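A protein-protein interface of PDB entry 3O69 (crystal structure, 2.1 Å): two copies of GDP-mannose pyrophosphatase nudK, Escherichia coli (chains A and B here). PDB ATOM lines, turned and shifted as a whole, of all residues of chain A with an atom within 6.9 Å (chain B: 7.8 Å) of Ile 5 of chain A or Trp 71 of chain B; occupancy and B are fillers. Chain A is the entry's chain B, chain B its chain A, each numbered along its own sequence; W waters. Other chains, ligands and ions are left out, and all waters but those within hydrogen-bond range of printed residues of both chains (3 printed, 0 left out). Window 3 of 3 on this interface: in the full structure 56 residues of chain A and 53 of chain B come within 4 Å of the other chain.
Water W2 lies within hydrogen-bond range of the backbone carbonyl oxygen of Ser 77 of chain B (2.7 Å), the backbone carbonyl oxygen of Gln 3 of chain A (2.9 Å) and the side-chain amide nitrogen of Gln 79 of chain B (3.2 Å). Water W3 lies within hydrogen-bond range of the backbone NH (N) of Phe 66 of chain B (2.9 Å) and the side-chain amide oxygen (OE1) of Gln 3 of chain A (3.2 Å). Water W1 lies within hydrogen-bond range of OH of Tyr 25 of chain A (3.0 Å), O of Phe 66 of chain B (3.0 Å) and N of Val 68 of chain B (3.1 Å).
Of the 14 printed residues of chain B, 9 touch a printed residue of chain A. Printed residues of chain B that touch a printed residue of chain A: Phe 66, Val 68, Thr 70, Trp 71, Val 72, Asn 73, Gly 74, Asn 75 and Gln 79. Of the 13 printed residues of chain A, 6 touch a printed residue of chain B. Printed residues of chain A that touch a printed residue of chain B: Gln 3, Ile 5, Ile 23, Tyr 25, Leu 27 and Tyr 119. Hydrophobic or aromatic side chains of chain A that line the printed part of chain B: Ile 5, Ile 23, Tyr 25, Leu 27 and Tyr 119.
Of chain B, only Phe 66 (3.3 Å) and Trp 71 (3.6 Å) come within 4 Å of Ile 5 of chain A. Printed residues of chain A within 4 Å of Trp 71 of chain B: Ile 5 (3.6 Å). Printed residues of chain A within 4 Å of Val 68 of chain B: Tyr 25. Printed residues of chain B within 4 Å of Leu 27 of chain A: Phe 66 (3.8 Å). Of the printed residues of chain A, Gly 74 of chain B touches Tyr 119. Of the printed residues of chain A, Val 72 of chain B touches Ile 23. Of the printed residues of chain A, Asn 75 of chain B touches Tyr 119. Gly 78 of chain B touches none of the printed residues of chain A. Thr 6 of chain A touches none of the printed residues of chain B. The nearest residue of chain B that does not touch Ile 5 of chain A is Ser 77 of chain B (4.3 Å). The nearest printed residue of chain A that does not touch Trp 71 of chain B is Leu 7 of chain A (4.001 Å).
Among the printed residues, pairs that only touch across the chains: Ile 5 of chain A with Phe 66 of chain B (3.3 Å), Tyr 25 of chain A with Phe 66 of chain B (3.5 Å), Tyr 119 of chain A with Gly 74 of chain B (3.5 Å), Ile 5 of chain A with Trp 71 of chain B (3.6 Å), Tyr 119 of chain A with Thr 70 of chain B (3.7 Å), Leu 27 of chain A with Phe 66 of chain B (3.8 Å), Tyr 25 of chain A with Val 68 of chain B (3.8 Å) and Ile 23 of chain A with Val 72 of chain B (3.9 Å).
The backbone carbonyl oxygen (O) of Asn 73 of chain B is in hydrogen-bond range of the side-chain hydroxyl (OH) of Tyr 119 of chain A (2.6 Å). The backbone NH (N) of Asn 75 of chain B is in hydrogen-bond range of the side-chain hydroxyl (OH) of Tyr 119 of chain A, at 3.3 Å. OE1 of Gln 3 of chain A is in hydrogen-bond range of NE2 of Gln 79 of chain B (2.8 Å).
No position is printed for both chains.
The backbone carbonyl oxygen (O) of Arg 67 of chain B lies within hydrogen-bond range of the side-chain hydroxyl (OG1) of Thr 70 of chain B (2.9 Å). OG1 of Thr 70 of chain B sits at hydrogen-bond distance from ND2 of Asn 75 of chain B (2.8 Å). The side-chain hydroxyl (OG1) of Thr 70 of chain B sits at hydrogen-bond distance from the backbone carbonyl oxygen (O) of Gly 78 of chain B. The side-chain amide nitrogen (ND2) of Asn 75 of chain B lies close to the backbone carbonyl oxygen (O) of Gly 78 of chain B (3.2 Å). ND2 of Asn 75 of chain B sits at hydrogen-bond distance from O of Gln 79 of chain B (2.9 Å). O of Thr 28 of chain A sits close to NE2 of Gln 3 of chain A (3.1 Å).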
ATOM      1  N   GLN A   3     -21.808 -25.293  -4.327  1.00  0.00           N
ATOM      2  CA  GLN A   3     -21.829 -23.886  -4.827  1.00  0.00           C
ATOM      3  C   GLN A   3     -21.212 -22.962  -3.764  1.00  0.00           C
ATOM      4  O   GLN A   3     -21.856 -22.647  -2.750  1.00  0.00           O
ATOM      5  CB  GLN A   3     -23.267 -23.480  -5.184  1.00  0.00           C
ATOM      6  CG  GLN A   3     -23.384 -22.256  -6.078  1.00  0.00           C
ATOM      7  CD  GLN A   3     -24.619 -22.264  -6.983  1.00  0.00           C
ATOM      8  OE1 GLN A   3     -25.764 -22.192  -6.516  1.00  0.00           O
ATOM      9  NE2 GLN A   3     -24.383 -22.307  -8.297  1.00  0.00           N
ATOM     10  N   GLN A   4     -19.957 -22.561  -3.986  1.00  0.00           N
ATOM     11  CA  GLN A   4     -19.274 -21.592  -3.125  1.00  0.00           C
ATOM     12  C   GLN A   4     -20.017 -20.258  -3.128  1.00  0.00           C
ATOM     13  O   GLN A   4     -20.370 -19.720  -4.184  1.00  0.00           O
ATOM     14  CB  GLN A   4     -17.802 -21.403  -3.536  1.00  0.00           C
ATOM     15  CG  GLN A   4     -17.050 -20.236  -2.839  1.00  0.00           C
ATOM     16  CD  GLN A   4     -16.720 -20.510  -1.362  1.00  0.00           C
ATOM     17  OE1 GLN A   4     -16.422 -21.647  -0.981  1.00  0.00           O
ATOM     18  NE2 GLN A   4     -16.766 -19.463  -0.532  1.00  0.00           N
ATOM     19  N   ILE A   5     -20.284 -19.755  -1.933  1.00  0.00           N
ATOM     20  CA  ILE A   5     -20.908 -18.459  -1.770  1.00  0.00           C
ATOM     21  C   ILE A   5     -19.997 -17.603  -0.907  1.00  0.00           C
ATOM     22  O   ILE A   5     -19.584 -18.029   0.162  1.00  0.00           O
ATOM     23  CB  ILE A   5     -22.360 -18.555  -1.166  1.00  0.00           C
ATOM     24  CG1 ILE A   5     -22.795 -17.214  -0.582  1.00  0.00           C
ATOM     25  CG2 ILE A   5     -22.473 -19.631  -0.083  1.00  0.00           C
ATOM     26  CD1 ILE A   5     -23.173 -16.225  -1.595  1.00  0.00           C
ATOM     27  N   THR A   6     -19.652 -16.413  -1.386  1.00  0.00           N
ATOM     28  CA  THR A   6     -18.861 -15.493  -0.568  1.00  0.00           C
ATOM     29  C   THR A   6     -19.445 -14.083  -0.535  1.00  0.00           C
ATOM     30  O   THR A   6     -19.710 -13.470  -1.582  1.00  0.00           O
ATOM     31  CB  THR A   6     -17.292 -15.504  -0.859  1.00  0.00           C
ATOM     32  OG1 THR A   6     -16.863 -14.268  -1.427  1.00  0.00           O
ATOM     33  CG2 THR A   6     -16.867 -16.621  -1.740  1.00  0.00           C
ATOM     34  N   LEU A   7     -19.675 -13.610   0.688  1.00  0.00           N
ATOM     35  CA  LEU A   7     -20.134 -12.242   0.943  1.00  0.00           C
ATOM     36  C   LEU A   7     -19.093 -11.210   0.525  1.00  0.00           C
ATOM     37  O   LEU A   7     -17.947 -11.263   0.965  1.00  0.00           O
ATOM     38  CB  LEU A   7     -20.483 -12.057   2.432  1.00  0.00           C
ATOM     39  CG  LEU A   7     -21.027 -10.690   2.872  1.00  0.00           C
ATOM     40  CD1 LEU A   7     -22.289 -10.363   2.110  1.00  0.00           C
ATOM     41  CD2 LEU A   7     -21.287 -10.691   4.386  1.00  0.00           C
ATOM     42  N   ILE A   8     -19.510 -10.250  -0.297  1.00  0.00           N
ATOM     43  CA  ILE A   8     -18.606  -9.215  -0.805  1.00  0.00           C
ATOM     44  C   ILE A   8     -18.829  -7.877  -0.100  1.00  0.00           C
ATOM     45  O   ILE A   8     -17.872  -7.197   0.291  1.00  0.00           O
ATOM     46  CB  ILE A   8     -18.751  -9.076  -2.357  1.00  0.00           C
ATOM     47  CG1 ILE A   8     -18.342 -10.386  -3.061  1.00  0.00           C
ATOM     48  CG2 ILE A   8     -17.992  -7.836  -2.907  1.00  0.00           C
ATOM     49  CD1 ILE A   8     -16.889 -10.831  -2.806  1.00  0.00           C
ATOM     50  N   ILE A  23     -27.184  -6.699  -0.331  1.00  0.00           N
ATOM     51  CA  ILE A  23     -26.097  -7.668  -0.217  1.00  0.00           C
ATOM     52  C   ILE A  23     -25.512  -8.002  -1.585  1.00  0.00           C
ATOM     53  O   ILE A  23     -26.235  -8.418  -2.495  1.00  0.00           O
ATOM     54  CB  ILE A  23     -26.530  -8.944   0.548  1.00  0.00           C
ATOM     55  CG1 ILE A  23     -27.126  -8.573   1.918  1.00  0.00           C
ATOM     56  CG2 ILE A  23     -25.342  -9.912   0.694  1.00  0.00           C
ATOM     57  CD1 ILE A  23     -27.583  -9.765   2.758  1.00  0.00           C
ATOM     58  N   THR A  24     -24.205  -7.768  -1.712  1.00  0.00           N
ATOM     59  CA  THR A  24     -23.416  -8.182  -2.881  1.00  0.00           C
ATOM     60  C   THR A  24     -22.732  -9.504  -2.533  1.00  0.00           C
ATOM     61  O   THR A  24     -22.103  -9.633  -1.487  1.00  0.00           O
ATOM     62  CB  THR A  24     -22.332  -7.137  -3.233  1.00  0.00           C
ATOM     63  OG1 THR A  24     -22.938  -5.848  -3.353  1.00  0.00           O
ATOM     64  CG2 THR A  24     -21.631  -7.490  -4.544  1.00  0.00           C
ATOM     65  N   TYR A  25     -22.889 -10.504  -3.386  1.00  0.00           N
ATOM     66  CA  TYR A  25     -22.274 -11.783  -3.109  1.00  0.00           C
ATOM     67  C   TYR A  25     -21.777 -12.404  -4.406  1.00  0.00           C
ATOM     68  O   TYR A  25     -22.278 -12.091  -5.494  1.00  0.00           O
ATOM     69  CB  TYR A  25     -23.235 -12.722  -2.333  1.00  0.00           C
ATOM     70  CG  TYR A  25     -24.496 -13.063  -3.090  1.00  0.00           C
ATOM     71  CD1 TYR A  25     -25.638 -12.272  -2.963  1.00  0.00           C
ATOM     72  CD2 TYR A  25     -24.547 -14.172  -3.946  1.00  0.00           C
ATOM     73  CE1 TYR A  25     -26.792 -12.573  -3.647  1.00  0.00           C
ATOM     74  CE2 TYR A  25     -25.697 -14.476  -4.648  1.00  0.00           C
ATOM     75  CZ  TYR A  25     -26.821 -13.680  -4.483  1.00  0.00           C
ATOM     76  OH  TYR A  25     -27.974 -13.965  -5.170  1.00  0.00           O
ATOM     77  N   ASP A  26     -20.759 -13.248  -4.260  1.00  0.00           N
ATOM     78  CA  ASP A  26     -20.205 -14.039  -5.332  1.00  0.00           C
ATOM     79  C   ASP A  26     -20.656 -15.488  -5.198  1.00  0.00           C
ATOM     80  O   ASP A  26     -20.524 -16.089  -4.138  1.00  0.00           O
ATOM     81  CB  ASP A  26     -18.669 -13.950  -5.306  1.00  0.00           C
ATOM     82  CG  ASP A  26     -18.146 -12.711  -6.016  1.00  0.00           C
ATOM     83  OD1 ASP A  26     -18.968 -11.978  -6.599  1.00  0.00           O
ATOM     84  OD2 ASP A  26     -16.921 -12.468  -5.998  1.00  0.00           O
ATOM     85  N   LEU A  27     -21.201 -16.030  -6.276  1.00  0.00           N
ATOM     86  CA  LEU A  27     -21.679 -17.395  -6.304  1.00  0.00           C
ATOM     87  C   LEU A  27     -20.979 -18.163  -7.428  1.00  0.00           C
ATOM     88  O   LEU A  27     -21.024 -17.743  -8.592  1.00  0.00           O
ATOM     89  CB  LEU A  27     -23.203 -17.387  -6.499  1.00  0.00           C
ATOM     90  CG  LEU A  27     -24.010 -18.660  -6.300  1.00  0.00           C
ATOM     91  CD1 LEU A  27     -23.925 -19.122  -4.834  1.00  0.00           C
ATOM     92  CD2 LEU A  27     -25.458 -18.425  -6.730  1.00  0.00           C
ATOM     93  N   THR A  28     -20.320 -19.269  -7.081  1.00  0.00           N
ATOM     94  CA  THR A  28     -19.628 -20.095  -8.073  1.00  0.00           C
ATOM     95  C   THR A  28     -20.564 -21.097  -8.769  1.00  0.00           C
ATOM     96  O   THR A  28     -21.297 -21.849  -8.122  1.00  0.00           O
ATOM     97  CB  THR A  28     -18.399 -20.822  -7.479  1.00  0.00           C
ATOM     98  OG1 THR A  28     -17.546 -19.866  -6.840  1.00  0.00           O
ATOM     99  CG2 THR A  28     -17.602 -21.508  -8.565  1.00  0.00           C
ATOM    100  N   TYR A 119     -39.552 -20.880   5.641  1.00  0.00           N
ATOM    101  CA  TYR A 119     -39.267 -19.584   5.062  1.00  0.00           C
ATOM    102  C   TYR A 119     -40.497 -19.221   4.229  1.00  0.00           C
ATOM    103  O   TYR A 119     -40.901 -19.987   3.354  1.00  0.00           O
ATOM    104  CB  TYR A 119     -37.998 -19.652   4.179  1.00  0.00           C
ATOM    105  CG  TYR A 119     -36.706 -19.906   4.940  1.00  0.00           C
ATOM    106  CD1 TYR A 119     -36.198 -18.944   5.812  1.00  0.00           C
ATOM    107  CD2 TYR A 119     -35.993 -21.112   4.785  1.00  0.00           C
ATOM    108  CE1 TYR A 119     -35.010 -19.166   6.525  1.00  0.00           C
ATOM    109  CE2 TYR A 119     -34.805 -21.341   5.478  1.00  0.00           C
ATOM    110  CZ  TYR A 119     -34.324 -20.361   6.346  1.00  0.00           C
ATOM    111  OH  TYR A 119     -33.160 -20.559   7.041  1.00  0.00           O
ATOM    112  N   PHE B  66     -29.948 -20.720  -4.942  1.00  0.00           N
ATOM    113  CA  PHE B  66     -29.425 -19.990  -3.796  1.00  0.00           C
ATOM    114  C   PHE B  66     -30.332 -18.819  -3.443  1.00  0.00           C
ATOM    115  O   PHE B  66     -30.635 -17.976  -4.295  1.00  0.00           O
ATOM    116  CB  PHE B  66     -28.007 -19.500  -4.088  1.00  0.00           C
ATOM    117  CG  PHE B  66     -27.400 -18.700  -2.973  1.00  0.00           C
ATOM    118  CD1 PHE B  66     -26.904 -19.322  -1.849  1.00  0.00           C
ATOM    119  CD2 PHE B  66     -27.306 -17.326  -3.070  1.00  0.00           C
ATOM    120  CE1 PHE B  66     -26.339 -18.579  -0.831  1.00  0.00           C
ATOM    121  CE2 PHE B  66     -26.749 -16.585  -2.064  1.00  0.00           C
ATOM    122  CZ  PHE B  66     -26.278 -17.213  -0.934  1.00  0.00           C
ATOM    123  N   ARG B  67     -30.781 -18.801  -2.191  1.00  0.00           N
ATOM    124  CA  ARG B  67     -31.553 -17.698  -1.650  1.00  0.00           C
ATOM    125  C   ARG B  67     -30.761 -17.065  -0.518  1.00  0.00           C
ATOM    126  O   ARG B  67     -30.670 -17.632   0.572  1.00  0.00           O
ATOM    127  CB  ARG B  67     -32.932 -18.184  -1.176  1.00  0.00           C
ATOM    128  CG  ARG B  67     -33.824 -18.745  -2.316  1.00  0.00           C
ATOM    129  CD  ARG B  67     -34.135 -17.676  -3.377  1.00  0.00           C
ATOM    130  NE  ARG B  67     -35.393 -17.970  -4.078  1.00  0.00           N
ATOM    131  CZ  ARG B  67     -35.952 -17.181  -4.992  1.00  0.00           C
ATOM    132  NH1 ARG B  67     -35.382 -16.030  -5.339  1.00  0.00           N
ATOM    133  NH2 ARG B  67     -37.102 -17.528  -5.549  1.00  0.00           N
ATOM    134  N   VAL B  68     -30.161 -15.905  -0.809  1.00  0.00           N
ATOM    135  CA  VAL B  68     -29.319 -15.166   0.137  1.00  0.00           C
ATOM    136  C   VAL B  68     -30.065 -14.773   1.421  1.00  0.00           C
ATOM    137  O   VAL B  68     -29.470 -14.686   2.481  1.00  0.00           O
ATOM    138  CB  VAL B  68     -28.635 -13.909  -0.543  1.00  0.00           C
ATOM    139  CG1 VAL B  68     -29.663 -12.861  -0.955  1.00  0.00           C
ATOM    140  CG2 VAL B  68     -27.567 -13.302   0.361  1.00  0.00           C
ATOM    141  N   ALA B  69     -31.373 -14.533   1.327  1.00  0.00           N
ATOM    142  CA  ALA B  69     -32.158 -14.159   2.497  1.00  0.00           C
ATOM    143  C   ALA B  69     -32.288 -15.335   3.471  1.00  0.00           C
ATOM    144  O   ALA B  69     -32.413 -15.139   4.681  1.00  0.00           O
ATOM    145  CB  ALA B  69     -33.534 -13.630   2.074  1.00  0.00           C
ATOM    146  N   THR B  70     -32.233 -16.559   2.948  1.00  0.00           N
ATOM    147  CA  THR B  70     -32.195 -17.752   3.821  1.00  0.00           C
ATOM    148  C   THR B  70     -30.764 -18.010   4.303  1.00  0.00           C
ATOM    149  O   THR B  70     -30.554 -18.448   5.445  1.00  0.00           O
ATOM    150  CB  THR B  70     -32.846 -19.006   3.158  1.00  0.00           C
ATOM    151  OG1 THR B  70     -31.952 -19.607   2.213  1.00  0.00           O
ATOM    152  CG2 THR B  70     -34.132 -18.621   2.442  1.00  0.00           C
ATOM    153  N   TRP B  71     -29.784 -17.676   3.465  1.00  0.00           N
ATOM    154  CA  TRP B  71     -28.360 -17.872   3.781  1.00  0.00           C
ATOM    155  C   TRP B  71     -27.885 -17.066   5.002  1.00  0.00           C
ATOM    156  O   TRP B  71     -27.100 -17.563   5.808  1.00  0.00           O
ATOM    157  CB  TRP B  71     -27.492 -17.546   2.553  1.00  0.00           C
ATOM    158  CG  TRP B  71     -26.025 -17.793   2.749  1.00  0.00           C
ATOM    159  CD1 TRP B  71     -25.409 -19.001   2.948  1.00  0.00           C
ATOM    160  CD2 TRP B  71     -24.984 -16.808   2.756  1.00  0.00           C
ATOM    161  NE1 TRP B  71     -24.054 -18.823   3.090  1.00  0.00           N
ATOM    162  CE2 TRP B  71     -23.762 -17.492   2.962  1.00  0.00           C
ATOM    163  CE3 TRP B  71     -24.965 -15.412   2.605  1.00  0.00           C
ATOM    164  CZ2 TRP B  71     -22.532 -16.830   3.029  1.00  0.00           C
ATOM    165  CZ3 TRP B  71     -23.729 -14.752   2.662  1.00  0.00           C
ATOM    166  CH2 TRP B  71     -22.536 -15.463   2.874  1.00  0.00           C
ATOM    167  N   VAL B  72     -28.348 -15.821   5.111  1.00  0.00           N
ATOM    168  CA  VAL B  72     -28.088 -14.983   6.285  1.00  0.00           C
ATOM    169  C   VAL B  72     -28.960 -15.346   7.504  1.00  0.00           C
ATOM    170  O   VAL B  72     -28.762 -14.789   8.584  1.00  0.00           O
ATOM    171  CB  VAL B  72     -28.256 -13.470   5.955  1.00  0.00           C
ATOM    172  CG1 VAL B  72     -27.218 -13.026   4.926  1.00  0.00           C
ATOM    173  CG2 VAL B  72     -29.672 -13.154   5.466  1.00  0.00           C
ATOM    174  N   ASN B  73     -29.926 -16.259   7.328  1.00  0.00           N
ATOM    175  CA  ASN B  73     -30.851 -16.611   8.411  1.00  0.00           C
ATOM    176  C   ASN B  73     -30.989 -18.136   8.626  1.00  0.00           C
ATOM    177  O   ASN B  73     -32.086 -18.687   8.514  1.00  0.00           O
ATOM    178  CB  ASN B  73     -32.234 -15.951   8.193  1.00  0.00           C
ATOM    179  CG  ASN B  73     -33.187 -16.155   9.380  1.00  0.00           C
ATOM    180  OD1 ASN B  73     -32.745 -16.274  10.524  1.00  0.00           O
ATOM    181  ND2 ASN B  73     -34.506 -16.181   9.106  1.00  0.00           N
ATOM    182  N   GLY B  74     -29.863 -18.801   8.886  1.00  0.00           N
ATOM    183  CA  GLY B  74     -29.856 -20.222   9.253  1.00  0.00           C
ATOM    184  C   GLY B  74     -29.895 -21.280   8.162  1.00  0.00           C
ATOM    185  O   GLY B  74     -29.898 -22.482   8.475  1.00  0.00           O
ATOM    186  N   ASN B  75     -29.928 -20.871   6.891  1.00  0.00           N
ATOM    187  CA  ASN B  75     -29.839 -21.847   5.803  1.00  0.00           C
ATOM    188  C   ASN B  75     -28.414 -21.968   5.291  1.00  0.00           C
ATOM    189  O   ASN B  75     -27.976 -21.207   4.424  1.00  0.00           O
ATOM    190  CB  ASN B  75     -30.824 -21.549   4.665  1.00  0.00           C
ATOM    191  CG  ASN B  75     -30.857 -22.649   3.600  1.00  0.00           C
ATOM    192  OD1 ASN B  75     -30.497 -23.804   3.855  1.00  0.00           O
ATOM    193  ND2 ASN B  75     -31.301 -22.292   2.404  1.00  0.00           N
ATOM    194  N   GLU B  76     -27.722 -22.971   5.820  1.00  0.00           N
ATOM    195  CA  GLU B  76     -26.270 -23.079   5.748  1.00  0.00           C
ATOM    196  C   GLU B  76     -25.662 -22.921   4.346  1.00  0.00           C
ATOM    197  O   GLU B  76     -24.695 -22.171   4.174  1.00  0.00           O
ATOM    198  CB  GLU B  76     -25.830 -24.390   6.400  1.00  0.00           C
ATOM    199  CG  GLU B  76     -24.341 -24.513   6.627  1.00  0.00           C
ATOM    200  CD  GLU B  76     -24.019 -25.651   7.580  1.00  0.00           C
ATOM    201  OE1 GLU B  76     -24.137 -25.433   8.811  1.00  0.00           O
ATOM    202  OE2 GLU B  76     -23.668 -26.758   7.093  1.00  0.00           O
ATOM    203  N   SER B  77     -26.222 -23.606   3.353  1.00  0.00           N
ATOM    204  CA  SER B  77     -25.731 -23.470   1.975  1.00  0.00           C
ATOM    205  C   SER B  77     -26.450 -22.377   1.173  1.00  0.00           C
ATOM    206  O   SER B  77     -26.054 -22.074   0.047  1.00  0.00           O
ATOM    207  CB  SER B  77     -25.844 -24.794   1.230  1.00  0.00           C
ATOM    208  OG  SER B  77     -27.193 -25.076   0.929  1.00  0.00           O
ATOM    209  N   GLY B  78     -27.516 -21.815   1.746  1.00  0.00           N
ATOM    210  CA  GLY B  78     -28.384 -20.901   1.033  1.00  0.00           C
ATOM    211  C   GLY B  78     -29.325 -21.589   0.058  1.00  0.00           C
ATOM    212  O   GLY B  78     -30.319 -20.995  -0.358  1.00  0.00           O
ATOM    213  N   GLN B  79     -29.025 -22.836  -0.311  1.00  0.00           N
ATOM    214  CA  GLN B  79     -29.834 -23.553  -1.308  1.00  0.00           C
ATOM    215  C   GLN B  79     -31.229 -23.865  -0.770  1.00  0.00           C
ATOM    216  O   GLN B  79     -31.374 -24.330   0.355  1.00  0.00           O
ATOM    217  CB  GLN B  79     -29.143 -24.839  -1.774  1.00  0.00           C
ATOM    218  CG  GLN B  79     -27.794 -24.631  -2.518  1.00  0.00           C
ATOM    219  CD  GLN B  79     -27.947 -23.932  -3.846  1.00  0.00           C
ATOM    220  OE1 GLN B  79     -28.943 -24.093  -4.543  1.00  0.00           O
ATOM    221  NE2 GLN B  79     -26.948 -23.147  -4.207  1.00  0.00           N
HETATM  222  O   HOH W   1     -30.323 -15.052  -3.734  1.00  0.00           O
HETATM  223  O   HOH W   2     -24.604 -23.130  -1.970  1.00  0.00           O
HETATM  224  O   HOH W   3     -28.363 -20.549  -7.412  1.00  0.00           O
